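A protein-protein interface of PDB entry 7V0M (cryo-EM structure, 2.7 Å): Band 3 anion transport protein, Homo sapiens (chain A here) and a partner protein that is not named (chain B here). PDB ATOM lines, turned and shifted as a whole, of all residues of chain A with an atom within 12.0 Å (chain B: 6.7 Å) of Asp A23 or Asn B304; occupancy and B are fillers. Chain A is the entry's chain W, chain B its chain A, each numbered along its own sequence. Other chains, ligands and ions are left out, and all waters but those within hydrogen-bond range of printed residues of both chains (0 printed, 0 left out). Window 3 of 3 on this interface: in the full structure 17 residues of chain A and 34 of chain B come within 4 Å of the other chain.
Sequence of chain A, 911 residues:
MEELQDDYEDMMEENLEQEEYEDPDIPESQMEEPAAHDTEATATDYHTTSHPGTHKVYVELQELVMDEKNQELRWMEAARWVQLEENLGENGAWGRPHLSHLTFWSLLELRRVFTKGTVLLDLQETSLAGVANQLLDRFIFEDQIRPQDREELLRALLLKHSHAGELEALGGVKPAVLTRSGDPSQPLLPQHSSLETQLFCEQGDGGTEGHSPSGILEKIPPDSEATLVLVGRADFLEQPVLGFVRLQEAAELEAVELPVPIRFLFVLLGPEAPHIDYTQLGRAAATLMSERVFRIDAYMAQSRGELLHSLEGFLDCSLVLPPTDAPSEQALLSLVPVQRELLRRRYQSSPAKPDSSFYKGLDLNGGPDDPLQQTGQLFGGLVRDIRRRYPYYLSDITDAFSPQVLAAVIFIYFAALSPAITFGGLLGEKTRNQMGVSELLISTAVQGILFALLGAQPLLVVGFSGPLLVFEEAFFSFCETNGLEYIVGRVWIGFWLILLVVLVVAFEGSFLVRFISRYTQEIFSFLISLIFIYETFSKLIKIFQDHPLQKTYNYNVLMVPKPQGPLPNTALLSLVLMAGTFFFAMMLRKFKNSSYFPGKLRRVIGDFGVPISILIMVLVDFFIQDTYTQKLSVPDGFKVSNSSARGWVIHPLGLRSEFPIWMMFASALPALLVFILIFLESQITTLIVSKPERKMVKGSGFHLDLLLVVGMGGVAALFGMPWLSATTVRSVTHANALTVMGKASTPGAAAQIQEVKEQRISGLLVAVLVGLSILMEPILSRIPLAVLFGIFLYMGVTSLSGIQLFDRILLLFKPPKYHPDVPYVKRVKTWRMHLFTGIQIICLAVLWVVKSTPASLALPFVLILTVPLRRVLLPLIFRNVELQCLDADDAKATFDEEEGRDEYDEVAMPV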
ATOM      1  N   GLU A  17     -35.650  14.551  34.212  1.00  0.00           N
ATOM      2  CA  GLU A  17     -34.278  14.378  33.727  1.00  0.00           C
ATOM      3  C   GLU A  17     -34.260  13.919  32.265  1.00  0.00           C
ATOM      4  O   GLU A  17     -33.850  12.807  31.930  1.00  0.00           O
ATOM      5  CB  GLU A  17     -33.498  13.407  34.621  1.00  0.00           C
ATOM      6  CG  GLU A  17     -33.483  13.786  36.086  1.00  0.00           C
ATOM      7  CD  GLU A  17     -32.611  12.869  36.915  1.00  0.00           C
ATOM      8  OE1 GLU A  17     -33.141  11.886  37.473  1.00  0.00           O
ATOM      9  OE2 GLU A  17     -31.393  13.129  37.009  1.00  0.00           O
ATOM     10  N   GLN A  18     -34.728  14.821  31.399  1.00  0.00           N
ATOM     11  CA  GLN A  18     -34.795  14.521  29.972  1.00  0.00           C
ATOM     12  C   GLN A  18     -33.415  14.282  29.371  1.00  0.00           C
ATOM     13  O   GLN A  18     -33.301  13.643  28.320  1.00  0.00           O
ATOM     14  CB  GLN A  18     -35.504  15.656  29.235  1.00  0.00           C
ATOM     15  CG  GLN A  18     -36.946  15.354  28.875  1.00  0.00           C
ATOM     16  CD  GLN A  18     -37.771  16.611  28.708  1.00  0.00           C
ATOM     17  OE1 GLN A  18     -38.138  17.258  29.688  1.00  0.00           O
ATOM     18  NE2 GLN A  18     -38.065  16.968  27.465  1.00  0.00           N
ATOM     19  N   GLU A  19     -32.359  14.788  30.015  1.00  0.00           N
ATOM     20  CA  GLU A  19     -31.008  14.579  29.506  1.00  0.00           C
ATOM     21  C   GLU A  19     -30.523  13.154  29.744  1.00  0.00           C
ATOM     22  O   GLU A  19     -29.561  12.715  29.105  1.00  0.00           O
ATOM     23  CB  GLU A  19     -30.047  15.580  30.145  1.00  0.00           C
ATOM     24  N   GLU A  20     -31.165  12.422  30.650  1.00  0.00           N
ATOM     25  CA  GLU A  20     -30.778  11.048  30.942  1.00  0.00           C
ATOM     26  C   GLU A  20     -31.333  10.048  29.936  1.00  0.00           C
ATOM     27  O   GLU A  20     -31.015   8.858  30.033  1.00  0.00           O
ATOM     28  CB  GLU A  20     -31.223  10.666  32.355  1.00  0.00           C
ATOM     29  CG  GLU A  20     -30.224  11.043  33.436  1.00  0.00           C
ATOM     30  CD  GLU A  20     -28.794  10.709  33.050  1.00  0.00           C
ATOM     31  OE1 GLU A  20     -28.472   9.507  32.932  1.00  0.00           O
ATOM     32  OE2 GLU A  20     -27.992  11.649  32.862  1.00  0.00           O
ATOM     33  N   TYR A  21     -32.157  10.493  28.987  1.00  0.00           N
ATOM     34  CA  TYR A  21     -32.665   9.644  27.918  1.00  0.00           C
ATOM     35  C   TYR A  21     -32.020   9.972  26.578  1.00  0.00           C
ATOM     36  O   TYR A  21     -32.601   9.692  25.525  1.00  0.00           O
ATOM     37  CB  TYR A  21     -34.187   9.757  27.818  1.00  0.00           C
ATOM     38  CG  TYR A  21     -34.905   9.420  29.104  1.00  0.00           C
ATOM     39  CD1 TYR A  21     -35.104  10.384  30.084  1.00  0.00           C
ATOM     40  CD2 TYR A  21     -35.377   8.137  29.344  1.00  0.00           C
ATOM     41  CE1 TYR A  21     -35.751  10.082  31.257  1.00  0.00           C
ATOM     42  CE2 TYR A  21     -36.027   7.826  30.517  1.00  0.00           C
ATOM     43  CZ  TYR A  21     -36.211   8.803  31.471  1.00  0.00           C
ATOM     44  OH  TYR A  21     -36.855   8.509  32.646  1.00  0.00           O
ATOM     45  N   GLU A  22     -30.829  10.562  26.600  1.00  0.00           N
ATOM     46  CA  GLU A  22     -30.135  10.986  25.396  1.00  0.00           C
ATOM     47  C   GLU A  22     -28.706  10.466  25.417  1.00  0.00           C
ATOM     48  O   GLU A  22     -28.132  10.230  26.481  1.00  0.00           O
ATOM     49  CB  GLU A  22     -30.126  12.514  25.269  1.00  0.00           C
ATOM     50  CG  GLU A  22     -31.462  13.113  24.874  1.00  0.00           C
ATOM     51  CD  GLU A  22     -31.458  14.627  24.936  1.00  0.00           C
ATOM     52  OE1 GLU A  22     -32.369  15.251  24.352  1.00  0.00           O
ATOM     53  OE2 GLU A  22     -30.544  15.193  25.571  1.00  0.00           O
ATOM     54  N   ASP A  23     -28.141  10.282  24.226  1.00  0.00           N
ATOM     55  CA  ASP A  23     -26.723   9.970  24.095  1.00  0.00           C
ATOM     56  C   ASP A  23     -25.924  11.251  24.291  1.00  0.00           C
ATOM     57  O   ASP A  23     -25.943  12.129  23.419  1.00  0.00           O
ATOM     58  CB  ASP A  23     -26.422   9.351  22.728  1.00  0.00           C
ATOM     59  CG  ASP A  23     -25.297   8.338  22.783  1.00  0.00           C
ATOM     60  OD1 ASP A  23     -24.142   8.744  23.039  1.00  0.00           O
ATOM     61  OD2 ASP A  23     -25.558   7.140  22.567  1.00  0.00           O
ATOM     62  N   PRO A  24     -25.220  11.401  25.421  1.00  0.00           N
ATOM     63  CA  PRO A  24     -24.560  12.681  25.718  1.00  0.00           C
ATOM     64  C   PRO A  24     -23.463  13.021  24.725  1.00  0.00           C
ATOM     65  O   PRO A  24     -23.517  14.065  24.065  1.00  0.00           O
ATOM     66  CB  PRO A  24     -23.988  12.466  27.127  1.00  0.00           C
ATOM     67  CG  PRO A  24     -24.643  11.213  27.645  1.00  0.00           C
ATOM     68  CD  PRO A  24     -24.931  10.385  26.443  1.00  0.00           C
ATOM     69  N   ASP A  25     -22.483  12.129  24.595  1.00  0.00           N
ATOM     70  CA  ASP A  25     -21.349  12.303  23.696  1.00  0.00           C
ATOM     71  C   ASP A  25     -20.518  11.030  23.725  1.00  0.00           C
ATOM     72  O   ASP A  25     -20.766  10.120  24.521  1.00  0.00           O
ATOM     73  CB  ASP A  25     -20.475  13.502  24.083  1.00  0.00           C
ATOM     74  N   ILE A  26     -19.524  10.984  22.845  1.00  0.00           N
ATOM     75  CA  ILE A  26     -18.518   9.926  22.843  1.00  0.00           C
ATOM     76  C   ILE A  26     -17.158  10.612  22.872  1.00  0.00           C
ATOM     77  O   ILE A  26     -16.511  10.746  21.822  1.00  0.00           O
ATOM     78  CB  ILE A  26     -18.664   9.003  21.625  1.00  0.00           C
ATOM     79  N   PRO A  27     -16.701  11.075  24.036  1.00  0.00           N
ATOM     80  CA  PRO A  27     -15.490  11.901  24.081  1.00  0.00           C
ATOM     81  C   PRO A  27     -14.250  11.128  23.661  1.00  0.00           C
ATOM     82  O   PRO A  27     -14.120   9.927  23.907  1.00  0.00           O
ATOM     83  CB  PRO A  27     -15.408  12.332  25.550  1.00  0.00           C
ATOM     84  CG  PRO A  27     -16.163  11.285  26.295  1.00  0.00           C
ATOM     85  CD  PRO A  27     -17.255  10.820  25.377  1.00  0.00           C
ATOM     86  N   GLU A  28     -13.334  11.841  23.017  1.00  0.00           N
ATOM     87  CA  GLU A  28     -12.068  11.282  22.562  1.00  0.00           C
ATOM     88  C   GLU A  28     -10.861  11.942  23.205  1.00  0.00           C
ATOM     89  O   GLU A  28      -9.852  11.268  23.437  1.00  0.00           O
ATOM     90  CB  GLU A  28     -11.956  11.398  21.035  1.00  0.00           C
ATOM     91  N   THR B 269     -35.975   6.442  21.468  1.00  0.00           N
ATOM     92  CA  THR B 269     -36.106   7.860  21.752  1.00  0.00           C
ATOM     93  C   THR B 269     -35.540   8.684  20.597  1.00  0.00           C
ATOM     94  O   THR B 269     -35.236   8.167  19.518  1.00  0.00           O
ATOM     95  CB  THR B 269     -35.409   8.208  23.065  1.00  0.00           C
ATOM     96  OG1 THR B 269     -33.997   8.011  22.928  1.00  0.00           O
ATOM     97  CG2 THR B 269     -35.929   7.334  24.195  1.00  0.00           C
ATOM     98  N   ASP B 271     -32.631  10.154  20.533  1.00  0.00           N
ATOM     99  CA  ASP B 271     -31.263   9.691  20.367  1.00  0.00           C
ATOM    100  C   ASP B 271     -31.172   8.179  20.198  1.00  0.00           C
ATOM    101  O   ASP B 271     -30.108   7.603  20.447  1.00  0.00           O
ATOM    102  CB  ASP B 271     -30.410  10.142  21.552  1.00  0.00           C
ATOM    103  CG  ASP B 271     -29.873  11.546  21.375  1.00  0.00           C
ATOM    104  OD1 ASP B 271     -30.156  12.163  20.327  1.00  0.00           O
ATOM    105  OD2 ASP B 271     -29.160  12.035  22.274  1.00  0.00           O
ATOM    106  N   GLU B 272     -32.266   7.533  19.791  1.00  0.00           N
ATOM    107  CA  GLU B 272     -32.339   6.112  19.457  1.00  0.00           C
ATOM    108  C   GLU B 272     -32.045   5.190  20.632  1.00  0.00           C
ATOM    109  O   GLU B 272     -31.453   4.125  20.442  1.00  0.00           O
ATOM    110  CB  GLU B 272     -31.407   5.765  18.291  1.00  0.00           C
ATOM    111  CG  GLU B 272     -32.116   5.568  16.970  1.00  0.00           C
ATOM    112  CD  GLU B 272     -31.166   5.625  15.794  1.00  0.00           C
ATOM    113  OE1 GLU B 272     -30.328   6.551  15.755  1.00  0.00           O
ATOM    114  OE2 GLU B 272     -31.252   4.745  14.913  1.00  0.00           O
ATOM    115  N   LEU B 273     -32.443   5.558  21.846  1.00  0.00           N
ATOM    116  CA  LEU B 273     -32.283   4.674  22.990  1.00  0.00           C
ATOM    117  C   LEU B 273     -33.529   3.821  23.187  1.00  0.00           C
ATOM    118  O   LEU B 273     -34.651   4.332  23.229  1.00  0.00           O
ATOM    119  CB  LEU B 273     -32.002   5.474  24.261  1.00  0.00           C
ATOM    120  CG  LEU B 273     -30.548   5.818  24.581  1.00  0.00           C
ATOM    121  CD1 LEU B 273     -30.075   6.995  23.749  1.00  0.00           C
ATOM    122  CD2 LEU B 273     -30.380   6.100  26.065  1.00  0.00           C
ATOM    123  N   HIS B 277     -31.556   0.139  26.741  1.00  0.00           N
ATOM    124  CA  HIS B 277     -30.476   1.110  26.904  1.00  0.00           C
ATOM    125  C   HIS B 277     -30.613   1.870  28.217  1.00  0.00           C
ATOM    126  O   HIS B 277     -29.628   2.064  28.936  1.00  0.00           O
ATOM    127  CB  HIS B 277     -30.461   2.092  25.733  1.00  0.00           C
ATOM    128  CG  HIS B 277     -29.695   1.609  24.543  1.00  0.00           C
ATOM    129  ND1 HIS B 277     -30.311   1.159  23.396  1.00  0.00           N
ATOM    130  CD2 HIS B 277     -28.364   1.516  24.317  1.00  0.00           C
ATOM    131  CE1 HIS B 277     -29.392   0.807  22.515  1.00  0.00           C
ATOM    132  NE2 HIS B 277     -28.202   1.013  23.050  1.00  0.00           N
ATOM    133  N   ARG B 281     -27.912   1.436  31.188  1.00  0.00           N
ATOM    134  CA  ARG B 281     -27.159   2.634  31.536  1.00  0.00           C
ATOM    135  C   ARG B 281     -27.189   2.901  33.035  1.00  0.00           C
ATOM    136  O   ARG B 281     -26.187   3.346  33.606  1.00  0.00           O
ATOM    137  CB  ARG B 281     -27.715   3.831  30.767  1.00  0.00           C
ATOM    138  CG  ARG B 281     -27.020   5.144  31.046  1.00  0.00           C
ATOM    139  CD  ARG B 281     -27.947   6.302  30.750  1.00  0.00           C
ATOM    140  NE  ARG B 281     -27.909   6.683  29.344  1.00  0.00           N
ATOM    141  CZ  ARG B 281     -27.736   7.923  28.909  1.00  0.00           C
ATOM    142  NH1 ARG B 281     -27.587   8.933  29.747  1.00  0.00           N
ATOM    143  NH2 ARG B 281     -27.714   8.153  27.600  1.00  0.00           N
ATOM    144  N   LYS B 301     -28.699  -0.127  18.738  1.00  0.00           N
ATOM    145  CA  LYS B 301     -27.679   0.906  18.804  1.00  0.00           C
ATOM    146  C   LYS B 301     -28.317   2.283  18.893  1.00  0.00           C
ATOM    147  O   LYS B 301     -29.412   2.508  18.370  1.00  0.00           O
ATOM    148  CB  LYS B 301     -26.755   0.836  17.588  1.00  0.00           C
ATOM    149  CG  LYS B 301     -25.522  -0.005  17.817  1.00  0.00           C
ATOM    150  CD  LYS B 301     -24.899  -0.446  16.513  1.00  0.00           C
ATOM    151  CE  LYS B 301     -23.389  -0.459  16.628  1.00  0.00           C
ATOM    152  NZ  LYS B 301     -22.970  -0.985  17.952  1.00  0.00           N
ATOM    153  N   THR B 302     -27.623   3.197  19.563  1.00  0.00           N
ATOM    154  CA  THR B 302     -28.044   4.587  19.647  1.00  0.00           C
ATOM    155  C   THR B 302     -27.523   5.340  18.423  1.00  0.00           C
ATOM    156  O   THR B 302     -27.061   4.740  17.449  1.00  0.00           O
ATOM    157  CB  THR B 302     -27.562   5.205  20.954  1.00  0.00           C
ATOM    158  OG1 THR B 302     -26.131   5.255  20.963  1.00  0.00           O
ATOM    159  CG2 THR B 302     -28.035   4.376  22.130  1.00  0.00           C
ATOM    160  N   LYS B 303     -27.595   6.674  18.454  1.00  0.00           N
ATOM    161  CA  LYS B 303     -27.138   7.455  17.309  1.00  0.00           C
ATOM    162  C   LYS B 303     -25.626   7.354  17.143  1.00  0.00           C
ATOM    163  O   LYS B 303     -25.110   7.466  16.026  1.00  0.00           O
ATOM    164  CB  LYS B 303     -27.558   8.919  17.448  1.00  0.00           C
ATOM    165  CG  LYS B 303     -26.945   9.641  18.634  1.00  0.00           C
ATOM    166  CD  LYS B 303     -27.430  11.072  18.723  1.00  0.00           C
ATOM    167  CE  LYS B 303     -26.822  11.778  19.921  1.00  0.00           C
ATOM    168  NZ  LYS B 303     -26.987  13.253  19.832  1.00  0.00           N
ATOM    169  N   ASN B 304     -24.902   7.139  18.241  1.00  0.00           N
ATOM    170  CA  ASN B 304     -23.452   7.009  18.218  1.00  0.00           C
ATOM    171  C   ASN B 304     -22.984   5.561  18.161  1.00  0.00           C
ATOM    172  O   ASN B 304     -21.789   5.308  18.335  1.00  0.00           O
ATOM    173  CB  ASN B 304     -22.838   7.697  19.438  1.00  0.00           C
ATOM    174  CG  ASN B 304     -23.193   9.164  19.518  1.00  0.00           C
ATOM    175  OD1 ASN B 304     -23.439   9.811  18.501  1.00  0.00           O
ATOM    176  ND2 ASN B 304     -23.212   9.701  20.730  1.00  0.00           N
ATOM    177  N   GLY B 305     -23.888   4.614  17.933  1.00  0.00           N
ATOM    178  CA  GLY B 305     -23.501   3.223  17.841  1.00  0.00           C
ATOM    179  C   GLY B 305     -23.251   2.534  19.161  1.00  0.00           C
ATOM    180  O   GLY B 305     -22.537   1.528  19.192  1.00  0.00           O
ATOM    181  N   LEU B 306     -23.817   3.036  20.254  1.00  0.00           N
ATOM    182  CA  LEU B 306     -23.646   2.415  21.560  1.00  0.00           C
ATOM    183  C   LEU B 306     -24.702   1.340  21.774  1.00  0.00           C
ATOM    184  O   LEU B 306     -25.902   1.620  21.723  1.00  0.00           O
ATOM    185  CB  LEU B 306     -23.729   3.454  22.677  1.00  0.00           C
ATOM    186  CG  LEU B 306     -22.414   4.073  23.151  1.00  0.00           C
ATOM    187  CD1 LEU B 306     -21.968   5.167  22.200  1.00  0.00           C
ATOM    188  CD2 LEU B 306     -22.543   4.600  24.570  1.00  0.00           C
ATOM    189  N   MET B 311     -23.301   1.040  27.462  1.00  0.00           N
ATOM    190  CA  MET B 311     -23.841   1.853  28.546  1.00  0.00           C
ATOM    191  C   MET B 311     -23.625   1.191  29.899  1.00  0.00           C
ATOM    192  O   MET B 311     -23.387   1.877  30.899  1.00  0.00           O
ATOM    193  CB  MET B 311     -25.325   2.128  28.310  1.00  0.00           C
ATOM    194  CG  MET B 311     -25.633   2.690  26.941  1.00  0.00           C
ATOM    195  SD  MET B 311     -26.771   4.080  27.010  1.00  0.00           S
ATOM    196  CE  MET B 311     -26.480   4.818  25.410  1.00  0.00           C
ATOM    197  N   GLN B 314     -20.016   1.782  30.745  1.00  0.00           N
ATOM    198  CA  GLN B 314     -19.735   3.183  31.037  1.00  0.00           C
ATOM    199  C   GLN B 314     -20.137   3.561  32.456  1.00  0.00           C
ATOM    200  O   GLN B 314     -19.523   4.448  33.056  1.00  0.00           O
ATOM    201  CB  GLN B 314     -20.451   4.076  30.026  1.00  0.00           C
ATOM    202  CG  GLN B 314     -19.739   5.384  29.745  1.00  0.00           C
ATOM    203  CD  GLN B 314     -20.574   6.326  28.909  1.00  0.00           C
ATOM    204  OE1 GLN B 314     -20.857   6.053  27.744  1.00  0.00           O
ATOM    205  NE2 GLN B 314     -20.978   7.442  29.500  1.00  0.00           N
ATOM    206  N   ILE B 334     -18.603  -2.377  18.467  1.00  0.00           N
ATOM    207  CA  ILE B 334     -17.921  -1.095  18.363  1.00  0.00           C
ATOM    208  C   ILE B 334     -18.953   0.004  18.167  1.00  0.00           C
ATOM    209  O   ILE B 334     -20.017  -0.223  17.581  1.00  0.00           O
ATOM    210  CB  ILE B 334     -16.896  -1.084  17.209  1.00  0.00           C
ATOM    211  CG1 ILE B 334     -17.528  -1.617  15.923  1.00  0.00           C
ATOM    212  CG2 ILE B 334     -15.673  -1.897  17.576  1.00  0.00           C
ATOM    213  CD1 ILE B 334     -17.111  -0.863  14.682  1.00  0.00           C
ATOM    214  N   THR B 335     -18.636   1.193  18.667  1.00  0.00           N
ATOM    215  CA  THR B 335     -19.438   2.375  18.407  1.00  0.00           C
ATOM    216  C   THR B 335     -19.044   2.978  17.060  1.00  0.00           C
ATOM    217  O   THR B 335     -18.293   2.388  16.281  1.00  0.00           O
ATOM    218  CB  THR B 335     -19.268   3.392  19.533  1.00  0.00           C
ATOM    219  OG1 THR B 335     -17.942   3.931  19.492  1.00  0.00           O
ATOM    220  CG2 THR B 335     -19.494   2.734  20.881  1.00  0.00           C
ATOM    221  N   LEU B 336     -19.561   4.175  16.777  1.00  0.00           N
ATOM    222  CA  LEU B 336     -19.159   4.867  15.558  1.00  0.00           C
ATOM    223  C   LEU B 336     -17.714   5.340  15.635  1.00  0.00           C
ATOM    224  O   LEU B 336     -17.055   5.490  14.601  1.00  0.00           O
ATOM    225  CB  LEU B 336     -20.096   6.039  15.279  1.00  0.00           C
ATOM    226  CG  LEU B 336     -21.492   5.652  14.791  1.00  0.00           C
ATOM    227  CD1 LEU B 336     -22.325   6.890  14.538  1.00  0.00           C
ATOM    228  CD2 LEU B 336     -21.406   4.798  13.540  1.00  0.00           C
ATOM    229  N   ASP B 337     -17.205   5.572  16.842  1.00  0.00           N
ATOM    230  CA  ASP B 337     -15.797   5.878  17.049  1.00  0.00           C
ATOM    231  C   ASP B 337     -14.945   4.628  17.225  1.00  0.00           C
ATOM    232  O   ASP B 337     -13.811   4.737  17.701  1.00  0.00           O
ATOM    233  CB  ASP B 337     -15.630   6.796  18.263  1.00  0.00           C
ATOM    234  CG  ASP B 337     -16.145   8.197  18.007  1.00  0.00           C
ATOM    235  OD1 ASP B 337     -15.397   9.163  18.265  1.00  0.00           O
ATOM    236  OD2 ASP B 337     -17.297   8.335  17.545  1.00  0.00           O
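OG1 of Thr B269 sits close to N of Asp B271, 3.5 Å away.
The side-chain hydroxyl (OG1) of Thr B269 is in hydrogen-bond range of the backbone NH (N) of Leu B273, 3.1 Å away.
The side-chain amino group of Lys B303 is in salt-bridge range of the side-chain carboxylate of Asp B271.
NE of Arg B281 is in hydrogen-bond range of SD of Met B311 (3.7 Å).
The side-chain hydroxyl of Thr B302 is in hydrogen-bond range of the backbone NH of Leu B306.
O of Asn B304 lies within hydrogen-bond range of N of Leu B336.
Of the 12 printed residues of chain A, 5 touch a printed residue of chain B.
Hydrophobic or aromatic side chains of chain A within 4 Å of the printed part of chain B: Pro A24.
Printed residues of chain B that touch a printed residue of chain A: Thr B269, Asp B271, Leu B273, Arg B281, Thr B302, Lys B303, Asn B304 and Met B311.
Hydrophobic or aromatic side chains of chain B that line the printed part of chain A: Leu B273 and Met B311.
Among the printed residues, Asp or Glu carboxylates within 4 Å of a Lys or Arg side-chain nitrogen of the other chain: Glu A20 with Arg B281 (3.4 Å).
Printed residues of chain B within 4 Å of Asp A23: Asp B271, Leu B273, Thr B302, Lys B303, Asn B304 and Met B311.
Of chain A, only Asp A23 comes within 4 Å of Asn B304.
Asp B271 touches two residues of chain A.
No residue of chain A comes within 4 Å of Glu B272.
Printed residues of chain A within 4 Å of Thr B302: Asp A23 (2.5 Å).
Lys B303 touches one residue of chain A.
No residue of chain A comes within 4 Å of Gly B305.
No residue of chain A comes within 4 Å of Leu B306.
Thr B335 touches none of the printed residues of chain A.
No residue of chain A comes within 4 Å of Leu B336.
Printed residues of chain B within 4 Å of Glu A22: Asp B271 (3.2 Å) and Arg B281 (2.4 Å).
Printed residues of chain A within 4 Å of Arg B281: Glu A20, Glu A22 and Pro A24.
Of the printed residues of chain A, Leu B273 touches Asp A23 (3.8 Å).
Asp A25 touches none of the printed residues of chain B.
The nearest printed residue of chain B that does not touch Asp A23 is Arg B281 (4.01 Å).
The nearest printed residue of chain A that does not touch Arg B281 is Asp A23 (4.01 Å).
CB of Glu A22 touches OD2 of Asp B271, 3.2 Å away.
N of Asp A23 touches CD1 of Leu B273, at 3.8 Å.
Lys B303 touches Asp A23 (CE to O, 3.6 Å).
OD2 of Asp A23 touches CE of Met B311, at 3.8 Å.
CD of Pro A24 touches NH2 of Arg B281, at 3.8 Å.
OG1 of Thr B269 sits at hydrogen-bond distance from O of Tyr A21 (3.4 Å).
The side-chain carboxylate of Asp B271 is in hydrogen-bond range of the backbone NH of Asp A23 (2.8 Å).
The guanidinium group (NH1) of Arg B281 is in salt-bridge range of the side-chain carboxylate (OE1) of Glu A20 (3.4 Å).
The side-chain hydroxyl of Thr B302 sits at hydrogen-bond distance from the side-chain carboxylate of Asp A23, at 2.5 Å.
The side-chain carboxylate (OD1) of Asp A23 sits at hydrogen-bond distance from the side-chain amide nitrogen (ND2) of Asn B304 (2.7 Å).
The backbone carbonyl oxygen of Glu A22 lies close to the guanidinium group of Arg B281, 2.4 Å away.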
